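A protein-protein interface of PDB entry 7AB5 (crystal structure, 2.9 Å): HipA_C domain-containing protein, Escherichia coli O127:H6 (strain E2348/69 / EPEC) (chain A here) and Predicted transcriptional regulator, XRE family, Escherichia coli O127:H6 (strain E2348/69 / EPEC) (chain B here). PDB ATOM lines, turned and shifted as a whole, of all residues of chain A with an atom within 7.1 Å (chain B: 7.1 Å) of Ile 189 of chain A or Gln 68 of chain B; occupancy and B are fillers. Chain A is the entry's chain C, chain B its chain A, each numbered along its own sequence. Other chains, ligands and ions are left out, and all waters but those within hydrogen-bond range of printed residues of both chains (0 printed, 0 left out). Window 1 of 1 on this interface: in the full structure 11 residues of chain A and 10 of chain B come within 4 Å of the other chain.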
ATOM      1  N   ASN A 186      24.835  -0.668  -8.427  1.00  0.00           N
ATOM      2  CA  ASN A 186      23.891   0.422  -8.631  1.00  0.00           C
ATOM      3  C   ASN A 186      24.040   1.434  -7.502  1.00  0.00           C
ATOM      4  O   ASN A 186      24.043   1.067  -6.323  1.00  0.00           O
ATOM      5  CB  ASN A 186      22.461  -0.113  -8.694  1.00  0.00           C
ATOM      6  CG  ASN A 186      21.481   0.907  -9.236  1.00  0.00           C
ATOM      7  OD1 ASN A 186      20.708   1.501  -8.485  1.00  0.00           O
ATOM      8  ND2 ASN A 186      21.511   1.118 -10.546  1.00  0.00           N
ATOM      9  N   ASP A 187      24.169   2.709  -7.864  1.00  0.00           N
ATOM     10  CA  ASP A 187      24.500   3.763  -6.904  1.00  0.00           C
ATOM     11  C   ASP A 187      23.268   4.387  -6.263  1.00  0.00           C
ATOM     12  O   ASP A 187      23.233   5.603  -6.056  1.00  0.00           O
ATOM     13  CB  ASP A 187      25.341   4.836  -7.588  1.00  0.00           C
ATOM     14  CG  ASP A 187      24.884   5.121  -9.004  1.00  0.00           C
ATOM     15  OD1 ASP A 187      24.035   4.366  -9.524  1.00  0.00           O
ATOM     16  OD2 ASP A 187      25.367   6.109  -9.594  1.00  0.00           O
ATOM     17  N   ASN A 188      22.244   3.600  -5.944  1.00  0.00           N
ATOM     18  CA  ASN A 188      21.101   4.157  -5.238  1.00  0.00           C
ATOM     19  C   ASN A 188      21.516   4.596  -3.838  1.00  0.00           C
ATOM     20  O   ASN A 188      22.445   4.045  -3.240  1.00  0.00           O
ATOM     21  CB  ASN A 188      19.959   3.141  -5.159  1.00  0.00           C
ATOM     22  CG  ASN A 188      20.418   1.778  -4.682  1.00  0.00           C
ATOM     23  OD1 ASN A 188      20.369   1.477  -3.490  1.00  0.00           O
ATOM     24  ND2 ASN A 188      20.846   0.937  -5.616  1.00  0.00           N
ATOM     25  N   ILE A 189      20.818   5.611  -3.319  1.00  0.00           N
ATOM     26  CA  ILE A 189      21.155   6.155  -2.005  1.00  0.00           C
ATOM     27  C   ILE A 189      21.014   5.093  -0.925  1.00  0.00           C
ATOM     28  O   ILE A 189      21.700   5.150   0.104  1.00  0.00           O
ATOM     29  CB  ILE A 189      20.284   7.391  -1.699  1.00  0.00           C
ATOM     30  CG1 ILE A 189      20.979   8.320  -0.702  1.00  0.00           C
ATOM     31  CG2 ILE A 189      18.894   6.989  -1.215  1.00  0.00           C
ATOM     32  CD1 ILE A 189      22.414   8.606  -1.055  1.00  0.00           C
ATOM     33  N   ALA A 190      20.135   4.110  -1.137  1.00  0.00           N
ATOM     34  CA  ALA A 190      19.979   3.037  -0.163  1.00  0.00           C
ATOM     35  C   ALA A 190      21.265   2.232  -0.029  1.00  0.00           C
ATOM     36  O   ALA A 190      21.664   1.865   1.082  1.00  0.00           O
ATOM     37  CB  ALA A 190      18.816   2.130  -0.561  1.00  0.00           C
ATOM     38  N   PHE A 191      21.933   1.959  -1.153  1.00  0.00           N
ATOM     39  CA  PHE A 191      23.197   1.234  -1.103  1.00  0.00           C
ATOM     40  C   PHE A 191      24.271   2.043  -0.390  1.00  0.00           C
ATOM     41  O   PHE A 191      25.036   1.500   0.416  1.00  0.00           O
ATOM     42  CB  PHE A 191      23.655   0.879  -2.516  1.00  0.00           C
ATOM     43  CG  PHE A 191      25.145   0.778  -2.654  1.00  0.00           C
ATOM     44  CD1 PHE A 191      25.827  -0.324  -2.167  1.00  0.00           C
ATOM     45  CD2 PHE A 191      25.868   1.795  -3.255  1.00  0.00           C
ATOM     46  CE1 PHE A 191      27.201  -0.414  -2.285  1.00  0.00           C
ATOM     47  CE2 PHE A 191      27.239   1.711  -3.375  1.00  0.00           C
ATOM     48  CZ  PHE A 191      27.907   0.605  -2.890  1.00  0.00           C
ATOM     49  N   LYS A 192      24.353   3.343  -0.683  1.00  0.00           N
ATOM     50  CA  LYS A 192      25.401   4.170  -0.096  1.00  0.00           C
ATOM     51  C   LYS A 192      25.226   4.298   1.412  1.00  0.00           C
ATOM     52  O   LYS A 192      26.209   4.268   2.162  1.00  0.00           O
ATOM     53  CB  LYS A 192      25.407   5.549  -0.752  1.00  0.00           C
ATOM     54  CG  LYS A 192      25.401   5.515  -2.267  1.00  0.00           C
ATOM     55  CD  LYS A 192      26.402   6.501  -2.839  1.00  0.00           C
ATOM     56  CE  LYS A 192      25.920   7.064  -4.165  1.00  0.00           C
ATOM     57  NZ  LYS A 192      26.143   8.533  -4.248  1.00  0.00           N
ATOM     58  N   ILE A 193      23.982   4.443   1.875  1.00  0.00           N
ATOM     59  CA  ILE A 193      23.737   4.592   3.305  1.00  0.00           C
ATOM     60  C   ILE A 193      24.101   3.311   4.046  1.00  0.00           C
ATOM     61  O   ILE A 193      24.726   3.354   5.113  1.00  0.00           O
ATOM     62  CB  ILE A 193      22.276   5.009   3.553  1.00  0.00           C
ATOM     63  CG1 ILE A 193      22.090   6.492   3.225  1.00  0.00           C
ATOM     64  CG2 ILE A 193      21.872   4.727   4.993  1.00  0.00           C
ATOM     65  CD1 ILE A 193      20.645   6.922   3.108  1.00  0.00           C
ATOM     66  N   ASP A 194      23.734   2.155   3.489  1.00  0.00           N
ATOM     67  CA  ASP A 194      24.105   0.884   4.106  1.00  0.00           C
ATOM     68  C   ASP A 194      25.619   0.740   4.201  1.00  0.00           C
ATOM     69  O   ASP A 194      26.156   0.373   5.253  1.00  0.00           O
ATOM     70  CB  ASP A 194      23.508  -0.281   3.318  1.00  0.00           C
ATOM     71  CG  ASP A 194      23.444  -1.562   4.132  1.00  0.00           C
ATOM     72  OD1 ASP A 194      24.206  -2.500   3.818  1.00  0.00           O
ATOM     73  OD2 ASP A 194      22.635  -1.630   5.084  1.00  0.00           O
ATOM     74  N   LEU A 195      26.324   1.018   3.101  1.00  0.00           N
ATOM     75  CA  LEU A 195      27.779   0.903   3.099  1.00  0.00           C
ATOM     76  C   LEU A 195      28.405   1.847   4.118  1.00  0.00           C
ATOM     77  O   LEU A 195      29.292   1.453   4.884  1.00  0.00           O
ATOM     78  CB  LEU A 195      28.319   1.185   1.697  1.00  0.00           C
ATOM     79  CG  LEU A 195      29.829   1.053   1.479  1.00  0.00           C
ATOM     80  CD1 LEU A 195      30.371  -0.231   2.089  1.00  0.00           C
ATOM     81  CD2 LEU A 195      30.158   1.128  -0.003  1.00  0.00           C
ATOM     82  N   MET A 285      31.098  10.120  -0.622  1.00  0.00           N
ATOM     83  CA  MET A 285      30.188   9.196  -1.288  1.00  0.00           C
ATOM     84  C   MET A 285      28.957   9.885  -1.855  1.00  0.00           C
ATOM     85  O   MET A 285      28.089   9.206  -2.413  1.00  0.00           O
ATOM     86  CB  MET A 285      29.741   8.081  -0.334  1.00  0.00           C
ATOM     87  CG  MET A 285      30.833   7.110   0.081  1.00  0.00           C
ATOM     88  SD  MET A 285      30.447   6.286   1.637  1.00  0.00           S
ATOM     89  CE  MET A 285      29.713   4.770   1.032  1.00  0.00           C
ATOM     90  N   GLY A 286      28.853  11.204  -1.724  1.00  0.00           N
ATOM     91  CA  GLY A 286      27.719  11.933  -2.249  1.00  0.00           C
ATOM     92  C   GLY A 286      26.578  12.147  -1.281  1.00  0.00           C
ATOM     93  O   GLY A 286      25.537  12.676  -1.689  1.00  0.00           O
ATOM     94  N   LEU A 287      26.732  11.752  -0.020  1.00  0.00           N
ATOM     95  CA  LEU A 287      25.677  11.968   0.962  1.00  0.00           C
ATOM     96  C   LEU A 287      25.600  13.444   1.331  1.00  0.00           C
ATOM     97  O   LEU A 287      26.609  14.057   1.696  1.00  0.00           O
ATOM     98  CB  LEU A 287      25.928  11.121   2.210  1.00  0.00           C
ATOM     99  CG  LEU A 287      26.089   9.611   2.019  1.00  0.00           C
ATOM    100  CD1 LEU A 287      26.481   8.944   3.327  1.00  0.00           C
ATOM    101  CD2 LEU A 287      24.816   8.997   1.477  1.00  0.00           C
ATOM    102  N   ALA A 288      24.403  14.014   1.233  1.00  0.00           N
ATOM    103  CA  ALA A 288      24.214  15.417   1.562  1.00  0.00           C
ATOM    104  C   ALA A 288      24.402  15.644   3.063  1.00  0.00           C
ATOM    105  O   ALA A 288      24.151  14.746   3.871  1.00  0.00           O
ATOM    106  CB  ALA A 288      22.828  15.886   1.131  1.00  0.00           C
ATOM    107  N   PRO A 289      24.849  16.841   3.460  1.00  0.00           N
ATOM    108  CA  PRO A 289      25.120  17.081   4.889  1.00  0.00           C
ATOM    109  C   PRO A 289      23.909  16.914   5.792  1.00  0.00           C
ATOM    110  O   PRO A 289      24.037  16.323   6.872  1.00  0.00           O
ATOM    111  CB  PRO A 289      25.642  18.524   4.895  1.00  0.00           C
ATOM    112  CG  PRO A 289      26.252  18.688   3.540  1.00  0.00           C
ATOM    113  CD  PRO A 289      25.305  17.965   2.625  1.00  0.00           C
ATOM    114  N   ARG A 290      22.736  17.422   5.395  1.00  0.00           N
ATOM    115  CA  ARG A 290      21.544  17.229   6.218  1.00  0.00           C
ATOM    116  C   ARG A 290      21.221  15.752   6.394  1.00  0.00           C
ATOM    117  O   ARG A 290      20.722  15.350   7.452  1.00  0.00           O
ATOM    118  CB  ARG A 290      20.343  17.968   5.620  1.00  0.00           C
ATOM    119  CG  ARG A 290      20.434  19.482   5.725  1.00  0.00           C
ATOM    120  CD  ARG A 290      19.155  20.193   5.275  1.00  0.00           C
ATOM    121  NE  ARG A 290      17.929  19.520   5.692  1.00  0.00           N
ATOM    122  CZ  ARG A 290      16.860  19.365   4.920  1.00  0.00           C
ATOM    123  NH1 ARG A 290      16.834  19.816   3.676  1.00  0.00           N
ATOM    124  NH2 ARG A 290      15.787  18.753   5.413  1.00  0.00           N
ATOM    125  N   LEU A 291      21.503  14.929   5.380  1.00  0.00           N
ATOM    126  CA  LEU A 291      21.316  13.489   5.531  1.00  0.00           C
ATOM    127  C   LEU A 291      22.344  12.896   6.484  1.00  0.00           C
ATOM    128  O   LEU A 291      22.012  12.032   7.304  1.00  0.00           O
ATOM    129  CB  LEU A 291      21.395  12.797   4.173  1.00  0.00           C
ATOM    130  CG  LEU A 291      21.252  11.275   4.262  1.00  0.00           C
ATOM    131  CD1 LEU A 291      19.818  10.897   4.602  1.00  0.00           C
ATOM    132  CD2 LEU A 291      21.709  10.592   2.982  1.00  0.00           C
ATOM    133  N   LEU A 292      23.598  13.341   6.389  1.00  0.00           N
ATOM    134  CA  LEU A 292      24.636  12.821   7.273  1.00  0.00           C
ATOM    135  C   LEU A 292      24.379  13.219   8.721  1.00  0.00           C
ATOM    136  O   LEU A 292      24.669  12.450   9.644  1.00  0.00           O
ATOM    137  CB  LEU A 292      26.006  13.309   6.807  1.00  0.00           C
ATOM    138  CG  LEU A 292      26.598  12.456   5.686  1.00  0.00           C
ATOM    139  CD1 LEU A 292      27.741  13.175   4.990  1.00  0.00           C
ATOM    140  CD2 LEU A 292      27.050  11.115   6.238  1.00  0.00           C
ATOM    141  N   LEU B  58      13.425  -0.228  -3.136  1.00  0.00           N
ATOM    142  CA  LEU B  58      14.696  -0.023  -2.457  1.00  0.00           C
ATOM    143  C   LEU B  58      14.532   0.288  -0.976  1.00  0.00           C
ATOM    144  O   LEU B  58      15.526   0.277  -0.242  1.00  0.00           O
ATOM    145  CB  LEU B  58      15.474   1.113  -3.126  1.00  0.00           C
ATOM    146  CG  LEU B  58      15.920   0.965  -4.580  1.00  0.00           C
ATOM    147  CD1 LEU B  58      16.458   2.290  -5.088  1.00  0.00           C
ATOM    148  CD2 LEU B  58      16.972  -0.121  -4.711  1.00  0.00           C
ATOM    149  N   ILE B  60      13.493   3.207   0.362  1.00  0.00           N
ATOM    150  CA  ILE B  60      13.721   4.609   0.693  1.00  0.00           C
ATOM    151  C   ILE B  60      12.379   5.285   0.933  1.00  0.00           C
ATOM    152  O   ILE B  60      11.431   5.105   0.158  1.00  0.00           O
ATOM    153  CB  ILE B  60      14.511   5.330  -0.415  1.00  0.00           C
ATOM    154  CG1 ILE B  60      15.917   4.753  -0.568  1.00  0.00           C
ATOM    155  CG2 ILE B  60      14.599   6.821  -0.141  1.00  0.00           C
ATOM    156  CD1 ILE B  60      16.215   4.283  -1.962  1.00  0.00           C
ATOM    157  N   LEU B  62      10.200   9.043   1.944  1.00  0.00           N
ATOM    158  CA  LEU B  62      10.211  10.401   1.413  1.00  0.00           C
ATOM    159  C   LEU B  62      11.135  11.310   2.214  1.00  0.00           C
ATOM    160  O   LEU B  62      11.780  12.200   1.649  1.00  0.00           O
ATOM    161  CB  LEU B  62       8.788  10.960   1.391  1.00  0.00           C
ATOM    162  CG  LEU B  62       7.822  10.214   0.469  1.00  0.00           C
ATOM    163  CD1 LEU B  62       6.460  10.886   0.451  1.00  0.00           C
ATOM    164  CD2 LEU B  62       8.395  10.112  -0.937  1.00  0.00           C
ATOM    165  N   TYR B  63      11.219  11.101   3.531  1.00  0.00           N
ATOM    166  CA  TYR B  63      12.063  11.961   4.355  1.00  0.00           C
ATOM    167  C   TYR B  63      13.542  11.767   4.042  1.00  0.00           C
ATOM    168  O   TYR B  63      14.315  12.730   4.105  1.00  0.00           O
ATOM    169  CB  TYR B  63      11.794  11.704   5.838  1.00  0.00           C
ATOM    170  CG  TYR B  63      12.450  12.709   6.762  1.00  0.00           C
ATOM    171  CD1 TYR B  63      12.669  14.020   6.353  1.00  0.00           C
ATOM    172  CD2 TYR B  63      12.847  12.348   8.043  1.00  0.00           C
ATOM    173  CE1 TYR B  63      13.269  14.941   7.192  1.00  0.00           C
ATOM    174  CE2 TYR B  63      13.446  13.263   8.891  1.00  0.00           C
ATOM    175  CZ  TYR B  63      13.655  14.559   8.460  1.00  0.00           C
ATOM    176  OH  TYR B  63      14.251  15.471   9.301  1.00  0.00           O
ATOM    177  N   THR B  64      13.957  10.543   3.708  1.00  0.00           N
ATOM    178  CA  THR B  64      15.344  10.328   3.303  1.00  0.00           C
ATOM    179  C   THR B  64      15.659  11.083   2.020  1.00  0.00           C
ATOM    180  O   THR B  64      16.729  11.688   1.893  1.00  0.00           O
ATOM    181  CB  THR B  64      15.627   8.835   3.124  1.00  0.00           C
ATOM    182  OG1 THR B  64      14.889   8.084   4.096  1.00  0.00           O
ATOM    183  CG2 THR B  64      17.115   8.548   3.283  1.00  0.00           C
ATOM    184  N   LEU B  65      14.732  11.063   1.058  1.00  0.00           N
ATOM    185  CA  LEU B  65      14.954  11.784  -0.190  1.00  0.00           C
ATOM    186  C   LEU B  65      15.000  13.291   0.034  1.00  0.00           C
ATOM    187  O   LEU B  65      15.786  13.989  -0.613  1.00  0.00           O
ATOM    188  CB  LEU B  65      13.875  11.431  -1.210  1.00  0.00           C
ATOM    189  CG  LEU B  65      13.927  10.042  -1.841  1.00  0.00           C
ATOM    190  CD1 LEU B  65      12.706   9.834  -2.717  1.00  0.00           C
ATOM    191  CD2 LEU B  65      15.204   9.858  -2.642  1.00  0.00           C
ATOM    192  N   GLU B  66      14.164  13.819   0.937  1.00  0.00           N
ATOM    193  CA  GLU B  66      14.201  15.258   1.198  1.00  0.00           C
ATOM    194  C   GLU B  66      15.560  15.688   1.737  1.00  0.00           C
ATOM    195  O   GLU B  66      16.074  16.749   1.368  1.00  0.00           O
ATOM    196  CB  GLU B  66      13.095  15.676   2.171  1.00  0.00           C
ATOM    197  CG  GLU B  66      12.950  17.203   2.270  1.00  0.00           C
ATOM    198  CD  GLU B  66      11.932  17.663   3.291  1.00  0.00           C
ATOM    199  OE1 GLU B  66      10.750  17.271   3.188  1.00  0.00           O
ATOM    200  OE2 GLU B  66      12.329  18.424   4.202  1.00  0.00           O
ATOM    201  N   LEU B  67      16.162  14.873   2.607  1.00  0.00           N
ATOM    202  CA  LEU B  67      17.451  15.240   3.186  1.00  0.00           C
ATOM    203  C   LEU B  67      18.572  15.152   2.157  1.00  0.00           C
ATOM    204  O   LEU B  67      19.481  15.992   2.147  1.00  0.00           O
ATOM    205  CB  LEU B  67      17.756  14.340   4.380  1.00  0.00           C
ATOM    206  CG  LEU B  67      16.761  14.426   5.533  1.00  0.00           C
ATOM    207  CD1 LEU B  67      16.997  13.290   6.489  1.00  0.00           C
ATOM    208  CD2 LEU B  67      16.887  15.755   6.253  1.00  0.00           C
ATOM    209  N   GLN B  68      18.532  14.137   1.292  1.00  0.00           N
ATOM    210  CA  GLN B  68      19.617  13.924   0.341  1.00  0.00           C
ATOM    211  C   GLN B  68      19.582  14.950  -0.781  1.00  0.00           C
ATOM    212  O   GLN B  68      20.630  15.432  -1.229  1.00  0.00           O
ATOM    213  CB  GLN B  68      19.528  12.510  -0.234  1.00  0.00           C
ATOM    214  CG  GLN B  68      20.511  12.226  -1.352  1.00  0.00           C
ATOM    215  CD  GLN B  68      21.944  12.532  -0.962  1.00  0.00           C
ATOM    216  OE1 GLN B  68      22.331  12.394   0.199  1.00  0.00           O
ATOM    217  NE2 GLN B  68      22.739  12.955  -1.936  1.00  0.00           N
ATOM    218  N   THR B  69      18.379  15.301  -1.230  1.00  0.00           N
ATOM    219  CA  THR B  69      18.135  16.069  -2.443  1.00  0.00           C
ATOM    220  C   THR B  69      17.686  17.492  -2.208  1.00  0.00           C
ATOM    221  O   THR B  69      18.032  18.370  -3.001  1.00  0.00           O
ATOM    222  CB  THR B  69      17.083  15.358  -3.299  1.00  0.00           C
ATOM    223  OG1 THR B  69      15.758  15.652  -2.808  1.00  0.00           O
ATOM    224  CG2 THR B  69      17.388  13.860  -3.345  1.00  0.00           C
ATOM    225  N   GLY B  70      16.924  17.740  -1.155  1.00  0.00           N
ATOM    226  CA  GLY B  70      16.429  19.064  -0.892  1.00  0.00           C
ATOM    227  C   GLY B  70      15.052  19.364  -1.439  1.00  0.00           C
ATOM    228  O   GLY B  70      14.516  20.438  -1.140  1.00  0.00           O
ATOM    229  N   ILE B  71      14.462  18.477  -2.242  1.00  0.00           N
ATOM    230  CA  ILE B  71      13.079  18.694  -2.652  1.00  0.00           C
ATOM    231  C   ILE B  71      12.155  18.289  -1.507  1.00  0.00           C
ATOM    232  O   ILE B  71      12.296  17.207  -0.924  1.00  0.00           O
ATOM    233  CB  ILE B  71      12.729  17.957  -3.968  1.00  0.00           C
ATOM    234  CG1 ILE B  71      13.755  18.112  -5.109  1.00  0.00           C
ATOM    235  CG2 ILE B  71      11.399  18.393  -4.491  1.00  0.00           C
ATOM    236  CD1 ILE B  71      14.609  16.879  -5.375  1.00  0.00           C
ATOM    237  N   ASN B  96      18.627  10.011 -10.173  1.00  0.00           N
ATOM    238  CA  ASN B  96      20.002   9.626  -9.870  1.00  0.00           C
ATOM    239  C   ASN B  96      20.105   9.001  -8.485  1.00  0.00           C
ATOM    240  O   ASN B  96      20.866   8.048  -8.280  1.00  0.00           O
ATOM    241  CB  ASN B  96      20.923  10.839  -9.979  1.00  0.00           C
ATOM    242  CG  ASN B  96      21.786  10.807 -11.222  1.00  0.00           C
ATOM    243  OD1 ASN B  96      21.319  10.459 -12.307  1.00  0.00           O
ATOM    244  ND2 ASN B  96      23.055  11.172 -11.071  1.00  0.00           N
ATOM    245  N   VAL B  97      19.348   9.532  -7.522  1.00  0.00           N
ATOM    246  CA  VAL B  97      19.346   9.001  -6.162  1.00  0.00           C
ATOM    247  C   VAL B  97      18.823   7.572  -6.130  1.00  0.00           C
ATOM    248  O   VAL B  97      19.209   6.778  -5.263  1.00  0.00           O
ATOM    249  CB  VAL B  97      18.524   9.928  -5.244  1.00  0.00           C
ATOM    250  CG1 VAL B  97      18.732   9.571  -3.803  1.00  0.00           C
ATOM    251  CG2 VAL B  97      18.934  11.365  -5.459  1.00  0.00           C
ATOM    252  N   LEU B  98      17.951   7.214  -7.069  1.00  0.00           N
ATOM    253  CA  LEU B  98      17.342   5.894  -7.107  1.00  0.00           C
ATOM    254  C   LEU B  98      18.093   4.916  -8.002  1.00  0.00           C
ATOM    255  O   LEU B  98      17.639   3.779  -8.172  1.00  0.00           O
ATOM    256  CB  LEU B  98      15.889   6.010  -7.572  1.00  0.00           C
ATOM    257  CG  LEU B  98      15.005   6.871  -6.666  1.00  0.00           C
ATOM    258  CD1 LEU B  98      13.656   7.138  -7.312  1.00  0.00           C
ATOM    259  CD2 LEU B  98      14.832   6.214  -5.306  1.00  0.00           C
ATOM    260  N   GLY B  99      19.225   5.323  -8.573  1.00  0.00           N
ATOM    261  CA  GLY B  99      19.965   4.452  -9.465  1.00  0.00           C
ATOM    262  C   GLY B  99      19.344   4.283 -10.830  1.00  0.00           C
ATOM    263  O   GLY B  99      19.638   3.302 -11.518  1.00  0.00           O
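The guanidinium group (NH2) of Arg 290 of chain A is in salt-bridge range of the side-chain carboxylate (OE2) of Glu 66 of chain B.
The side-chain amide nitrogen (NE2) of Gln 68 of chain B is in hydrogen-bond range of the backbone carbonyl oxygen (O) of Gly 286 of chain A (2.8 Å).
The side-chain amide oxygen (OE1) of Gln 68 of chain B lies within hydrogen-bond range of the backbone NH (N) of Ala 288 of chain A (2.8 Å).
O of Val 97 of chain B is in hydrogen-bond range of N of Ile 189 of chain A (2.8 Å).
O of Gly 99 of chain B sits at hydrogen-bond distance from ND2 of Asn 186 of chain A, 3.0 Å away.
The side-chain amide oxygen (OD1) of Asn 186 of chain A is in hydrogen-bond range of the side-chain amide nitrogen (ND2) of Asn 188 of chain A (2.9 Å).
The backbone NH (N) of Phe 191 of chain A sits at hydrogen-bond distance from the side-chain amide oxygen (OD1) of Asn 188 of chain A (2.9 Å).
Leu 98 of chain B touches Asn 186 of chain A (O to OD1, 3.8 Å).
CD1 of Leu 58 of chain B touches CB of Asn 188 of chain A (3.6 Å).
Ile 189 of chain A touches Ile 60 of chain B (CG2 to CG1, 3.8 Å).
Ile 189 of chain A touches Gln 68 of chain B (CD1 to CD, 3.96 Å).
O of Leu 58 of chain B touches CB of Ala 190 of chain A, at 3.8 Å.
CD1 of Ile 60 of chain B touches CB of Ala 190 of chain A, at 3.7 Å.
Ile 193 of chain A touches Thr 64 of chain B.
Gln 68 of chain B touches Leu 287 of chain A.
Ala 288 of chain A touches Leu 67 of chain B.
Arg 290 of chain A touches Leu 67 of chain B (NH2 to CD2, 3.3 Å).
Pro 289 of chain A touches none of the printed residues of chain B.
Of the printed residues of chain B, Leu 291 of chain A touches Thr 64 (3.8 Å), Leu 67 (3.8 Å) and Gln 68 (3.4 Å).
Leu 62 of chain B touches none of the printed residues of chain A.
Of the printed residues of chain A, Leu 67 of chain B touches Ala 288, Arg 290 and Leu 291.
Of chain A, only Ile 189 (3.96 Å), Gly 286 (2.8 Å), Leu 287 (3.5 Å), Ala 288 (2.8 Å) and Leu 291 (3.4 Å) come within 4 Å of Gln 68 of chain B.
The nearest residue of chain B that does not touch Ile 189 of chain A is Leu 65 of chain B (4.9 Å).
Of the 16 printed residues of chain B, 9 touch a printed residue of chain A.
Hydrophobic or aromatic side chains of chain B that line the printed part of chain A: Leu 58, Ile 60, Leu 67 and Val 97.
Along chain B the printed residues that touch a printed residue of chain A span positions 58 to 99.
Of the 18 printed residues of chain A, 10 touch a printed residue of chain B.
Hydrophobic or aromatic side chains of chain A that line the printed part of chain B: Ile 189, Ala 190, Ile 193, Ala 288 and Leu 291.
Among the printed residues, 20 pairs touch across the chains.
Among the printed residues, Asp or Glu carboxylates within 4 Å of a Lys or Arg side-chain nitrogen of the other chain: Arg 290 of chain A with Glu 66 of chain B (3.7 Å).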
